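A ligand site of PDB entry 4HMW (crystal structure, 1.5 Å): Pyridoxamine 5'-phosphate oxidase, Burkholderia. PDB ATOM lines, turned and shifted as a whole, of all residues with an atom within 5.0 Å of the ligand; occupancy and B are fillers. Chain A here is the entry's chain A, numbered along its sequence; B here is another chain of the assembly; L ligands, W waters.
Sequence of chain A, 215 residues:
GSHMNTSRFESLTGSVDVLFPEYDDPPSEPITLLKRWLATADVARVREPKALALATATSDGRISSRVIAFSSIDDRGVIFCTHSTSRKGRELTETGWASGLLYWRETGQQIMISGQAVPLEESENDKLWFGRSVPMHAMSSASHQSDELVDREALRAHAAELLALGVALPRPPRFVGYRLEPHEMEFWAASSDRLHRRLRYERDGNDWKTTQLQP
OE1 of Glu 48 touches C7 of the ligand (3.7 Å).
Ile 68 touches the ligand (CD1 to N2, 3.6 Å).
Tyr 103 of chain B touches the ligand.
Hydrophobic or aromatic side chains within 4 Å of the ligand: Val 67, Ile 68, Ala 69, Tyr 103 of chain B and Trp 188 of chain B.
16 residues have an atom within 4 Å of the ligand: Glu 48, Arg 66, Val 67, Ile 68, Ala 69, Cys 81, Thr 82, Ser 86, Arg 87, Lys 88, Gln 145, Ser 146, Tyr 103 of chain B, Gln 110 of chain B, Trp 188 of chain B and Arg 198 of chain B.
The guanidinium group (NH1) of Arg 198 of chain B is in hydrogen-bond range of the side-chain hydroxyl (OG) of Ser 146.
The backbone NH (N) of Val 67 sits at hydrogen-bond distance from the side-chain amide oxygen (OE1) of Gln 110 of chain B, at 2.9 Å.
The side-chain amino group (NZ) of Lys 88 sits at hydrogen-bond distance from the side-chain hydroxyl (OG1) of Thr 82 (2.9 Å).
The guanidinium group (NE) of Arg 198 of chain B is in salt-bridge range of the side-chain carboxylate (OE2) of Glu 186 of chain B (2.8 Å).
N of Gln 110 of chain B is in hydrogen-bond range of O of Trp 188 of chain B, 3.0 Å away.
The side-chain amide oxygen (OE1) of Gln 145 sits at hydrogen-bond distance from the backbone NH (N) of His 83 (3.4 Å).
The side-chain amide nitrogen of Gln 145 sits at hydrogen-bond distance from the chain-end carboxylate of Pro 215 of chain B, 3.2 Å away.
The side-chain hydroxyl (OG) of Ser 86 lies within hydrogen-bond range of the backbone NH (N) of Gly 89, 3.0 Å away.
O8 of the ligand lies within hydrogen-bond range of OG of Ser 146 (2.5 Å).
An oxygen (O3) of the ligand sits at hydrogen-bond distance from the backbone NH (N) of Val 67 (3.4 Å).
The backbone carbonyl oxygen (O) of Val 67 is in hydrogen-bond range of an oxygen (O3) of the ligand (2.7 Å).
N of Lys 88 is in hydrogen-bond range of O7 of the ligand.
An oxygen (O7) of the ligand lies within salt-bridge range of the side-chain amino group (NZ) of Lys 88 (2.8 Å).
The side-chain hydroxyl (OG1) of Thr 82 lies within hydrogen-bond range of an oxygen (O1) of the ligand.
NH1 of Arg 66 lies within salt-bridge range of O9 of the ligand, at 2.8 Å.
The backbone carbonyl oxygen of Cys 81 lies within hydrogen-bond range of a nitrogen (N2) of the ligand.
An oxygen (O8) of the ligand is in salt-bridge range of the guanidinium group (NH2) of Arg 198 of chain B, at 2.9 Å.
The side-chain amide nitrogen (NE2) of Gln 110 of chain B is in hydrogen-bond range of an oxygen (O3) of the ligand, at 2.9 Å.
An oxygen (O1) of the ligand lies within hydrogen-bond range of the side-chain amide nitrogen of Gln 145 (3.1 Å).
N3 of the ligand sits at hydrogen-bond distance from N of Ala 69 (3.2 Å).
N of Arg 87 lies within hydrogen-bond range of O7 of the ligand, 3.2 Å away.
NE1 of Trp 188 of chain B lies within hydrogen-bond range of O4 of the ligand, 3.4 Å away.
OG of Ser 86 lies within hydrogen-bond range of O7 of the ligand.
Water W6 bridges O9 of the ligand (2.6 Å) and O of Ser 65 (3.2 Å).
Water W3 lies within hydrogen-bond range of O2 of the ligand (2.8 Å), N of Cys 81 (2.9 Å) and O of Ala 69 (3.0 Å).
Water W11 lies within hydrogen-bond range of NH2 of Arg 200 of chain B, O8 of the ligand and NH1 of Arg 87.
Water W5 bridges O4 of the ligand and OE1 of Glu 186 of chain B.
Water W7 lies within hydrogen-bond range of an oxygen (O2) of the ligand and the backbone carbonyl oxygen (O) of Ala 69.
Water W2 bridges SG of Cys 81 (2.9 Å) and O2 of the ligand (3.3 Å).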
ATOM      1  N   GLU A  48      -6.560  11.876 -24.154  1.00  0.00           N
ATOM      2  CA  GLU A  48      -7.404  13.086 -24.142  1.00  0.00           C
ATOM      3  C   GLU A  48      -6.732  14.321 -24.740  1.00  0.00           C
ATOM      4  O   GLU A  48      -6.508  15.334 -24.056  1.00  0.00           O
ATOM      5  CB  GLU A  48      -7.852  13.390 -22.706  1.00  0.00           C
ATOM      6  CG  GLU A  48      -8.790  12.338 -22.139  1.00  0.00           C
ATOM      7  CD  GLU A  48      -9.278  12.665 -20.743  1.00  0.00           C
ATOM      8  OE1 GLU A  48      -9.536  13.865 -20.443  1.00  0.00           O
ATOM      9  OE2 GLU A  48      -9.389  11.723 -19.913  1.00  0.00           O
ATOM     10  N   ALA A  51      -8.479  17.935 -24.475  1.00  0.00           N
ATOM     11  CA  ALA A  51      -8.766  18.540 -23.169  1.00  0.00           C
ATOM     12  C   ALA A  51      -8.053  19.884 -23.073  1.00  0.00           C
ATOM     13  O   ALA A  51      -6.849  19.970 -22.821  1.00  0.00           O
ATOM     14  CB  ALA A  51      -8.359  17.610 -22.027  1.00  0.00           C
ATOM     15  N   SER A  65     -10.374  29.389 -14.725  1.00  0.00           N
ATOM     16  CA  SER A  65      -9.979  28.329 -15.652  1.00  0.00           C
ATOM     17  C   SER A  65     -10.733  27.030 -15.380  1.00  0.00           C
ATOM     18  O   SER A  65     -11.127  26.780 -14.245  1.00  0.00           O
ATOM     19  CB  SER A  65      -8.475  28.010 -15.548  1.00  0.00           C
ATOM     20  OG  SER A  65      -7.676  29.141 -15.736  1.00  0.00           O
ATOM     21  N   ARG A  66     -10.903  26.221 -16.417  1.00  0.00           N
ATOM     22  CA  ARG A  66     -11.468  24.876 -16.288  1.00  0.00           C
ATOM     23  C   ARG A  66     -11.141  24.084 -17.541  1.00  0.00           C
ATOM     24  O   ARG A  66     -10.912  24.679 -18.618  1.00  0.00           O
ATOM     25  CB  ARG A  66     -13.000  24.887 -16.094  1.00  0.00           C
ATOM     26  CG  ARG A  66     -13.828  25.268 -17.306  1.00  0.00           C
ATOM     27  CD  ARG A  66     -13.545  26.676 -17.742  1.00  0.00           C
ATOM     28  NE  ARG A  66     -14.077  27.603 -16.811  1.00  0.00           N
ATOM     29  CZ  ARG A  66     -13.796  28.912 -16.798  1.00  0.00           C
ATOM     30  NH1 ARG A  66     -14.395  29.670 -15.906  1.00  0.00           N
ATOM     31  NH2 ARG A  66     -12.949  29.468 -17.662  1.00  0.00           N
ATOM     32  N   VAL A  67     -11.178  22.753 -17.441  1.00  0.00           N
ATOM     33  CA  VAL A  67     -11.024  21.898 -18.625  1.00  0.00           C
ATOM     34  C   VAL A  67     -12.292  21.893 -19.478  1.00  0.00           C
ATOM     35  O   VAL A  67     -13.404  21.785 -18.947  1.00  0.00           O
ATOM     36  CB  VAL A  67     -10.677  20.462 -18.234  1.00  0.00           C
ATOM     37  CG1 VAL A  67     -10.551  19.581 -19.471  1.00  0.00           C
ATOM     38  CG2 VAL A  67      -9.411  20.439 -17.416  1.00  0.00           C
ATOM     39  N   ILE A  68     -12.105  22.003 -20.781  1.00  0.00           N
ATOM     40  CA  ILE A  68     -13.175  21.831 -21.770  1.00  0.00           C
ATOM     41  C   ILE A  68     -12.683  20.878 -22.863  1.00  0.00           C
ATOM     42  O   ILE A  68     -11.606  21.066 -23.406  1.00  0.00           O
ATOM     43  CB  ILE A  68     -13.505  23.173 -22.444  1.00  0.00           C
ATOM     44  CG1 ILE A  68     -13.992  24.164 -21.411  1.00  0.00           C
ATOM     45  CG2 ILE A  68     -14.564  23.024 -23.568  1.00  0.00           C
ATOM     46  CD1 ILE A  68     -15.389  23.893 -20.910  1.00  0.00           C
ATOM     47  N   ALA A  69     -13.430  19.836 -23.141  1.00  0.00           N
ATOM     48  CA  ALA A  69     -13.113  18.989 -24.269  1.00  0.00           C
ATOM     49  C   ALA A  69     -13.801  19.599 -25.482  1.00  0.00           C
ATOM     50  O   ALA A  69     -15.018  19.499 -25.635  1.00  0.00           O
ATOM     51  CB  ALA A  69     -13.603  17.578 -24.024  1.00  0.00           C
ATOM     52  N   CYS A  81     -18.978  23.666 -26.230  1.00  0.00           N
ATOM     53  CA  CYS A  81     -20.300  23.929 -25.689  1.00  0.00           C
ATOM     54  C   CYS A  81     -20.261  23.958 -24.166  1.00  0.00           C
ATOM     55  O   CYS A  81     -19.373  23.367 -23.525  1.00  0.00           O
ATOM     56  CB  CYS A  81     -21.307  22.902 -26.202  1.00  0.00           C
ATOM     57  SG  CYS A  81     -20.906  21.200 -25.780  1.00  0.00           S
ATOM     58  N   THR A  82     -21.222  24.679 -23.602  1.00  0.00           N
ATOM     59  CA  THR A  82     -21.314  24.823 -22.163  1.00  0.00           C
ATOM     60  C   THR A  82     -22.691  25.411 -21.792  1.00  0.00           C
ATOM     61  O   THR A  82     -23.553  25.582 -22.669  1.00  0.00           O
ATOM     62  CB  THR A  82     -20.169  25.736 -21.665  1.00  0.00           C
ATOM     63  OG1 THR A  82     -20.096  25.653 -20.260  1.00  0.00           O
ATOM     64  CG2 THR A  82     -20.402  27.170 -22.071  1.00  0.00           C
ATOM     65  N   HIS A  83     -22.922  25.683 -20.505  1.00  0.00           N
ATOM     66  CA  HIS A  83     -24.158  26.339 -20.068  1.00  0.00           C
ATOM     67  C   HIS A  83     -23.927  27.837 -20.034  1.00  0.00           C
ATOM     68  O   HIS A  83     -22.918  28.301 -19.488  1.00  0.00           O
ATOM     69  CB  HIS A  83     -24.603  25.874 -18.679  1.00  0.00           C
ATOM     70  CG  HIS A  83     -25.089  24.445 -18.629  1.00  0.00           C
ATOM     71  ND1 HIS A  83     -26.008  24.002 -17.710  1.00  0.00           N
ATOM     72  CD2 HIS A  83     -24.732  23.368 -19.344  1.00  0.00           C
ATOM     73  CE1 HIS A  83     -26.239  22.719 -17.902  1.00  0.00           C
ATOM     74  NE2 HIS A  83     -25.466  22.302 -18.882  1.00  0.00           N
ATOM     75  N   SER A  86     -23.487  29.250 -16.536  1.00  0.00           N
ATOM     76  CA  SER A  86     -22.312  28.857 -15.800  1.00  0.00           C
ATOM     77  C   SER A  86     -21.415  30.058 -15.541  1.00  0.00           C
ATOM     78  O   SER A  86     -21.594  31.142 -16.102  1.00  0.00           O
ATOM     79  CB  SER A  86     -21.527  27.784 -16.545  1.00  0.00           C
ATOM     80  OG  SER A  86     -20.885  28.285 -17.698  1.00  0.00           O
ATOM     81  N   ARG A  87     -20.408  29.847 -14.716  1.00  0.00           N
ATOM     82  CA  ARG A  87     -19.473  30.905 -14.400  1.00  0.00           C
ATOM     83  C   ARG A  87     -18.701  31.351 -15.650  1.00  0.00           C
ATOM     84  O   ARG A  87     -18.550  32.557 -15.883  1.00  0.00           O
ATOM     85  CB  ARG A  87     -18.562  30.454 -13.266  1.00  0.00           C
ATOM     86  CG  ARG A  87     -17.643  31.508 -12.686  1.00  0.00           C
ATOM     87  CD  ARG A  87     -16.267  31.338 -13.189  1.00  0.00           C
ATOM     88  NE  ARG A  87     -15.382  32.250 -12.492  1.00  0.00           N
ATOM     89  CZ  ARG A  87     -14.902  32.033 -11.263  1.00  0.00           C
ATOM     90  NH1 ARG A  87     -15.190  30.905 -10.627  1.00  0.00           N
ATOM     91  NH2 ARG A  87     -14.129  32.914 -10.698  1.00  0.00           N
ATOM     92  N   LYS A  88     -18.270  30.402 -16.479  1.00  0.00           N
ATOM     93  CA  LYS A  88     -17.539  30.734 -17.704  1.00  0.00           C
ATOM     94  C   LYS A  88     -18.502  31.377 -18.681  1.00  0.00           C
ATOM     95  O   LYS A  88     -18.148  32.256 -19.451  1.00  0.00           O
ATOM     96  CB  LYS A  88     -16.871  29.509 -18.322  1.00  0.00           C
ATOM     97  CG  LYS A  88     -17.746  28.715 -19.295  1.00  0.00           C
ATOM     98  CD  LYS A  88     -17.134  27.396 -19.684  1.00  0.00           C
ATOM     99  CE  LYS A  88     -17.120  26.430 -18.538  1.00  0.00           C
ATOM    100  NZ  LYS A  88     -18.504  26.264 -17.962  1.00  0.00           N
ATOM    101  N   GLY A  89     -19.738  30.940 -18.646  1.00  0.00           N
ATOM    102  CA  GLY A  89     -20.739  31.511 -19.521  1.00  0.00           C
ATOM    103  C   GLY A  89     -20.922  32.986 -19.275  1.00  0.00           C
ATOM    104  O   GLY A  89     -21.034  33.792 -20.205  1.00  0.00           O
ATOM    105  N   GLN A 145     -25.363  24.255 -14.284  1.00  0.00           N
ATOM    106  CA  GLN A 145     -23.937  24.231 -14.128  1.00  0.00           C
ATOM    107  C   GLN A 145     -23.398  25.424 -13.365  1.00  0.00           C
ATOM    108  O   GLN A 145     -23.643  26.569 -13.719  1.00  0.00           O
ATOM    109  CB  GLN A 145     -23.284  24.101 -15.517  1.00  0.00           C
ATOM    110  CG  GLN A 145     -21.799  23.866 -15.505  1.00  0.00           C
ATOM    111  CD  GLN A 145     -21.237  23.747 -16.922  1.00  0.00           C
ATOM    112  OE1 GLN A 145     -21.270  24.700 -17.710  1.00  0.00           O
ATOM    113  NE2 GLN A 145     -20.767  22.535 -17.266  1.00  0.00           N
ATOM    114  N   SER A 146     -22.681  25.124 -12.291  1.00  0.00           N
ATOM    115  CA  SER A 146     -21.997  26.131 -11.479  1.00  0.00           C
ATOM    116  C   SER A 146     -22.851  26.888 -10.445  1.00  0.00           C
ATOM    117  O   SER A 146     -22.298  27.611  -9.616  1.00  0.00           O
ATOM    118  CB  SER A 146     -21.133  27.091 -12.321  1.00  0.00           C
ATOM    119  OG  SER A 146     -20.347  26.329 -13.181  1.00  0.00           O
ATOM    120  N   TYR B 103      -4.789  19.411 -14.128  1.00  0.00           N
ATOM    121  CA  TYR B 103      -5.743  18.409 -14.570  1.00  0.00           C
ATOM    122  C   TYR B 103      -5.036  17.108 -14.711  1.00  0.00           C
ATOM    123  O   TYR B 103      -4.063  16.988 -15.467  1.00  0.00           O
ATOM    124  CB  TYR B 103      -6.459  18.778 -15.903  1.00  0.00           C
ATOM    125  CG  TYR B 103      -7.277  17.635 -16.461  1.00  0.00           C
ATOM    126  CD1 TYR B 103      -8.180  16.966 -15.641  1.00  0.00           C
ATOM    127  CD2 TYR B 103      -7.211  17.265 -17.818  1.00  0.00           C
ATOM    128  CE1 TYR B 103      -8.949  15.909 -16.132  1.00  0.00           C
ATOM    129  CE2 TYR B 103      -7.984  16.202 -18.322  1.00  0.00           C
ATOM    130  CZ  TYR B 103      -8.844  15.540 -17.468  1.00  0.00           C
ATOM    131  OH  TYR B 103      -9.581  14.478 -17.933  1.00  0.00           O
ATOM    132  N   GLN B 110      -9.424  17.942 -11.342  1.00  0.00           N
ATOM    133  CA  GLN B 110      -8.841  19.221 -11.719  1.00  0.00           C
ATOM    134  C   GLN B 110      -8.819  20.142 -10.484  1.00  0.00           C
ATOM    135  O   GLN B 110      -9.606  19.998  -9.566  1.00  0.00           O
ATOM    136  CB  GLN B 110      -9.510  19.878 -12.959  1.00  0.00           C
ATOM    137  CG  GLN B 110     -10.906  20.070 -12.871  1.00  0.00           C
ATOM    138  CD  GLN B 110     -11.583  20.708 -14.124  1.00  0.00           C
ATOM    139  OE1 GLN B 110     -11.058  21.592 -14.806  1.00  0.00           O
ATOM    140  NE2 GLN B 110     -12.810  20.278 -14.360  1.00  0.00           N
ATOM    141  N   GLU B 186     -10.965  25.864  -6.799  1.00  0.00           N
ATOM    142  CA  GLU B 186     -11.981  24.835  -6.946  1.00  0.00           C
ATOM    143  C   GLU B 186     -11.322  23.507  -7.109  1.00  0.00           C
ATOM    144  O   GLU B 186     -10.289  23.372  -7.826  1.00  0.00           O
ATOM    145  CB  GLU B 186     -12.898  25.030  -8.182  1.00  0.00           C
ATOM    146  CG  GLU B 186     -14.000  23.906  -8.197  1.00  0.00           C
ATOM    147  CD  GLU B 186     -14.807  23.707  -9.502  1.00  0.00           C
ATOM    148  OE1 GLU B 186     -14.902  24.660 -10.346  1.00  0.00           O
ATOM    149  OE2 GLU B 186     -15.392  22.597  -9.656  1.00  0.00           O
ATOM    150  N   TRP B 188     -12.291  19.685  -8.276  1.00  0.00           N
ATOM    151  CA  TRP B 188     -13.272  18.944  -9.093  1.00  0.00           C
ATOM    152  C   TRP B 188     -12.857  17.490  -9.243  1.00  0.00           C
ATOM    153  O   TRP B 188     -11.720  17.208  -9.572  1.00  0.00           O
ATOM    154  CB  TRP B 188     -13.317  19.585 -10.463  1.00  0.00           C
ATOM    155  CG  TRP B 188     -14.310  19.074 -11.490  1.00  0.00           C
ATOM    156  CD1 TRP B 188     -15.499  19.651 -11.810  1.00  0.00           C
ATOM    157  CD2 TRP B 188     -14.197  17.936 -12.344  1.00  0.00           C
ATOM    158  NE1 TRP B 188     -16.123  18.974 -12.818  1.00  0.00           N
ATOM    159  CE2 TRP B 188     -15.341  17.933 -13.191  1.00  0.00           C
ATOM    160  CE3 TRP B 188     -13.219  16.963 -12.536  1.00  0.00           C
ATOM    161  CZ2 TRP B 188     -15.553  16.956 -14.154  1.00  0.00           C
ATOM    162  CZ3 TRP B 188     -13.421  16.006 -13.527  1.00  0.00           C
ATOM    163  CH2 TRP B 188     -14.580  16.014 -14.319  1.00  0.00           C
ATOM    164  N   ARG B 198     -17.756  18.984  -6.869  1.00  0.00           N
ATOM    165  CA  ARG B 198     -17.204  20.322  -7.096  1.00  0.00           C
ATOM    166  C   ARG B 198     -17.223  21.090  -5.810  1.00  0.00           C
ATOM    167  O   ARG B 198     -18.279  21.335  -5.253  1.00  0.00           O
ATOM    168  CB  ARG B 198     -18.040  21.087  -8.125  1.00  0.00           C
ATOM    169  CG  ARG B 198     -18.120  20.425  -9.521  1.00  0.00           C
ATOM    170  CD  ARG B 198     -18.769  21.379 -10.497  1.00  0.00           C
ATOM    171  NE  ARG B 198     -17.951  22.571 -10.695  1.00  0.00           N
ATOM    172  CZ  ARG B 198     -18.321  23.645 -11.408  1.00  0.00           C
ATOM    173  NH1 ARG B 198     -19.512  23.701 -11.973  1.00  0.00           N
ATOM    174  NH2 ARG B 198     -17.465  24.672 -11.531  1.00  0.00           N
ATOM    175  N   ARG B 200     -15.848  24.558  -4.103  1.00  0.00           N
ATOM    176  CA  ARG B 200     -15.289  25.884  -4.286  1.00  0.00           C
ATOM    177  C   ARG B 200     -14.925  26.541  -2.965  1.00  0.00           C
ATOM    178  O   ARG B 200     -15.713  26.531  -2.029  1.00  0.00           O
ATOM    179  CB  ARG B 200     -16.288  26.786  -5.045  1.00  0.00           C
ATOM    180  CG  ARG B 200     -15.888  28.249  -5.041  1.00  0.00           C
ATOM    181  CD  ARG B 200     -16.938  29.163  -5.647  1.00  0.00           C
ATOM    182  NE  ARG B 200     -17.172  28.958  -7.065  1.00  0.00           N
ATOM    183  CZ  ARG B 200     -18.292  29.337  -7.704  1.00  0.00           C
ATOM    184  NH1 ARG B 200     -19.297  29.890  -7.024  1.00  0.00           N
ATOM    185  NH2 ARG B 200     -18.409  29.133  -9.018  1.00  0.00           N
ATOM    186  N   PRO B 215     -22.684  20.306 -11.437  1.00  0.00           N
ATOM    187  CA  PRO B 215     -21.761  19.945 -12.508  1.00  0.00           C
ATOM    188  C   PRO B 215     -22.115  20.475 -13.887  1.00  0.00           C
ATOM    189  O   PRO B 215     -21.174  20.616 -14.733  1.00  0.00           O
ATOM    190  CB  PRO B 215     -21.853  18.429 -12.556  1.00  0.00           C
ATOM    191  CG  PRO B 215     -23.211  18.098 -12.014  1.00  0.00           C
ATOM    192  CD  PRO B 215     -23.477  19.155 -10.967  1.00  0.00           C
ATOM    193  OXT PRO B 215     -23.305  20.753 -14.194  1.00  0.00           O
HETATM  194  N1  LIG L   1     -17.767  21.624 -19.150  1.00  0.00           N
HETATM  195  C1  LIG L   1     -18.522  22.152 -20.161  1.00  0.00           C
HETATM  196  O1  LIG L   1     -19.352  23.006 -19.928  1.00  0.00           O
HETATM  197  N2  LIG L   1     -18.296  21.762 -21.456  1.00  0.00           N
HETATM  198  C2  LIG L   1     -17.363  20.794 -21.743  1.00  0.00           C
HETATM  199  O2  LIG L   1     -17.196  20.465 -22.930  1.00  0.00           O
HETATM  200  C3  LIG L   1     -16.619  20.231 -20.721  1.00  0.00           C
HETATM  201  N3  LIG L   1     -15.701  19.229 -20.980  1.00  0.00           N
HETATM  202  C4  LIG L   1     -14.946  18.722 -19.922  1.00  0.00           C
HETATM  203  C5  LIG L   1     -14.008  17.743 -20.190  1.00  0.00           C
HETATM  204  C6  LIG L   1     -13.222  17.234 -19.172  1.00  0.00           C
HETATM  205  C7  LIG L   1     -12.224  16.185 -19.512  1.00  0.00           C
HETATM  206  C8  LIG L   1     -13.410  17.678 -17.865  1.00  0.00           C
HETATM  207  C9  LIG L   1     -12.555  17.156 -16.748  1.00  0.00           C
HETATM  208  C10 LIG L   1     -14.341  18.654 -17.590  1.00  0.00           C
HETATM  209  C11 LIG L   1     -15.153  19.142 -18.607  1.00  0.00           C
HETATM  210  N4  LIG L   1     -16.139  20.131 -18.363  1.00  0.00           N
HETATM  211  C12 LIG L   1     -16.846  20.651 -19.416  1.00  0.00           C
HETATM  212  C13 LIG L   1     -16.447  20.674 -17.006  1.00  0.00           C
HETATM  213  C14 LIG L   1     -15.667  21.959 -16.730  1.00  0.00           C
HETATM  214  O3  LIG L   1     -14.279  21.673 -16.441  1.00  0.00           O
HETATM  215  C15 LIG L   1     -16.247  22.760 -15.574  1.00  0.00           C
HETATM  216  O4  LIG L   1     -16.274  21.928 -14.432  1.00  0.00           O
HETATM  217  C16 LIG L   1     -17.642  23.312 -15.906  1.00  0.00           C
HETATM  218  O5  LIG L   1     -17.732  23.573 -17.294  1.00  0.00           O
HETATM  219  C17 LIG L   1     -17.997  24.510 -15.047  1.00  0.00           C
HETATM  220  O6  LIG L   1     -17.012  25.515 -15.162  1.00  0.00           O
HETATM  221  P1  LIG L   1     -17.259  27.003 -14.647  1.00  0.00           P
HETATM  222  O7  LIG L   1     -18.215  27.681 -15.618  1.00  0.00           O
HETATM  223  O8  LIG L   1     -17.890  26.908 -13.254  1.00  0.00           O
HETATM  224  O9  LIG L   1     -15.932  27.655 -14.688  1.00  0.00           O
HETATM  225  O   HOH W   1     -18.074  17.638 -17.503  1.00  0.00           O
HETATM  226  O   HOH W   2     -20.456  19.846 -23.224  1.00  0.00           O
HETATM  227  O   HOH W   3     -17.331  21.362 -25.556  1.00  0.00           O
HETATM  228  O   HOH W   4     -18.940  17.901 -22.556  1.00  0.00           O
HETATM  229  O   HOH W   5     -14.315  23.133 -12.804  1.00  0.00           O
HETATM  230  O   HOH W   6     -13.991  27.444 -13.030  1.00  0.00           O
HETATM  231  O   HOH W   7     -17.211  17.893 -24.295  1.00  0.00           O
HETATM  232  O   HOH W   8     -21.783  21.261 -21.180  1.00  0.00           O
HETATM  233  O   HOH W   9     -16.184  15.695 -17.952  1.00  0.00           O
HETATM  234  O   HOH W  10     -11.273  14.950 -22.562  1.00  0.00           O
HETATM  235  O   HOH W  11     -16.801  28.387 -11.132  1.00  0.00           O
HETATM  236  O   HOH W  12     -18.502  20.163 -13.966  1.00  0.00           O
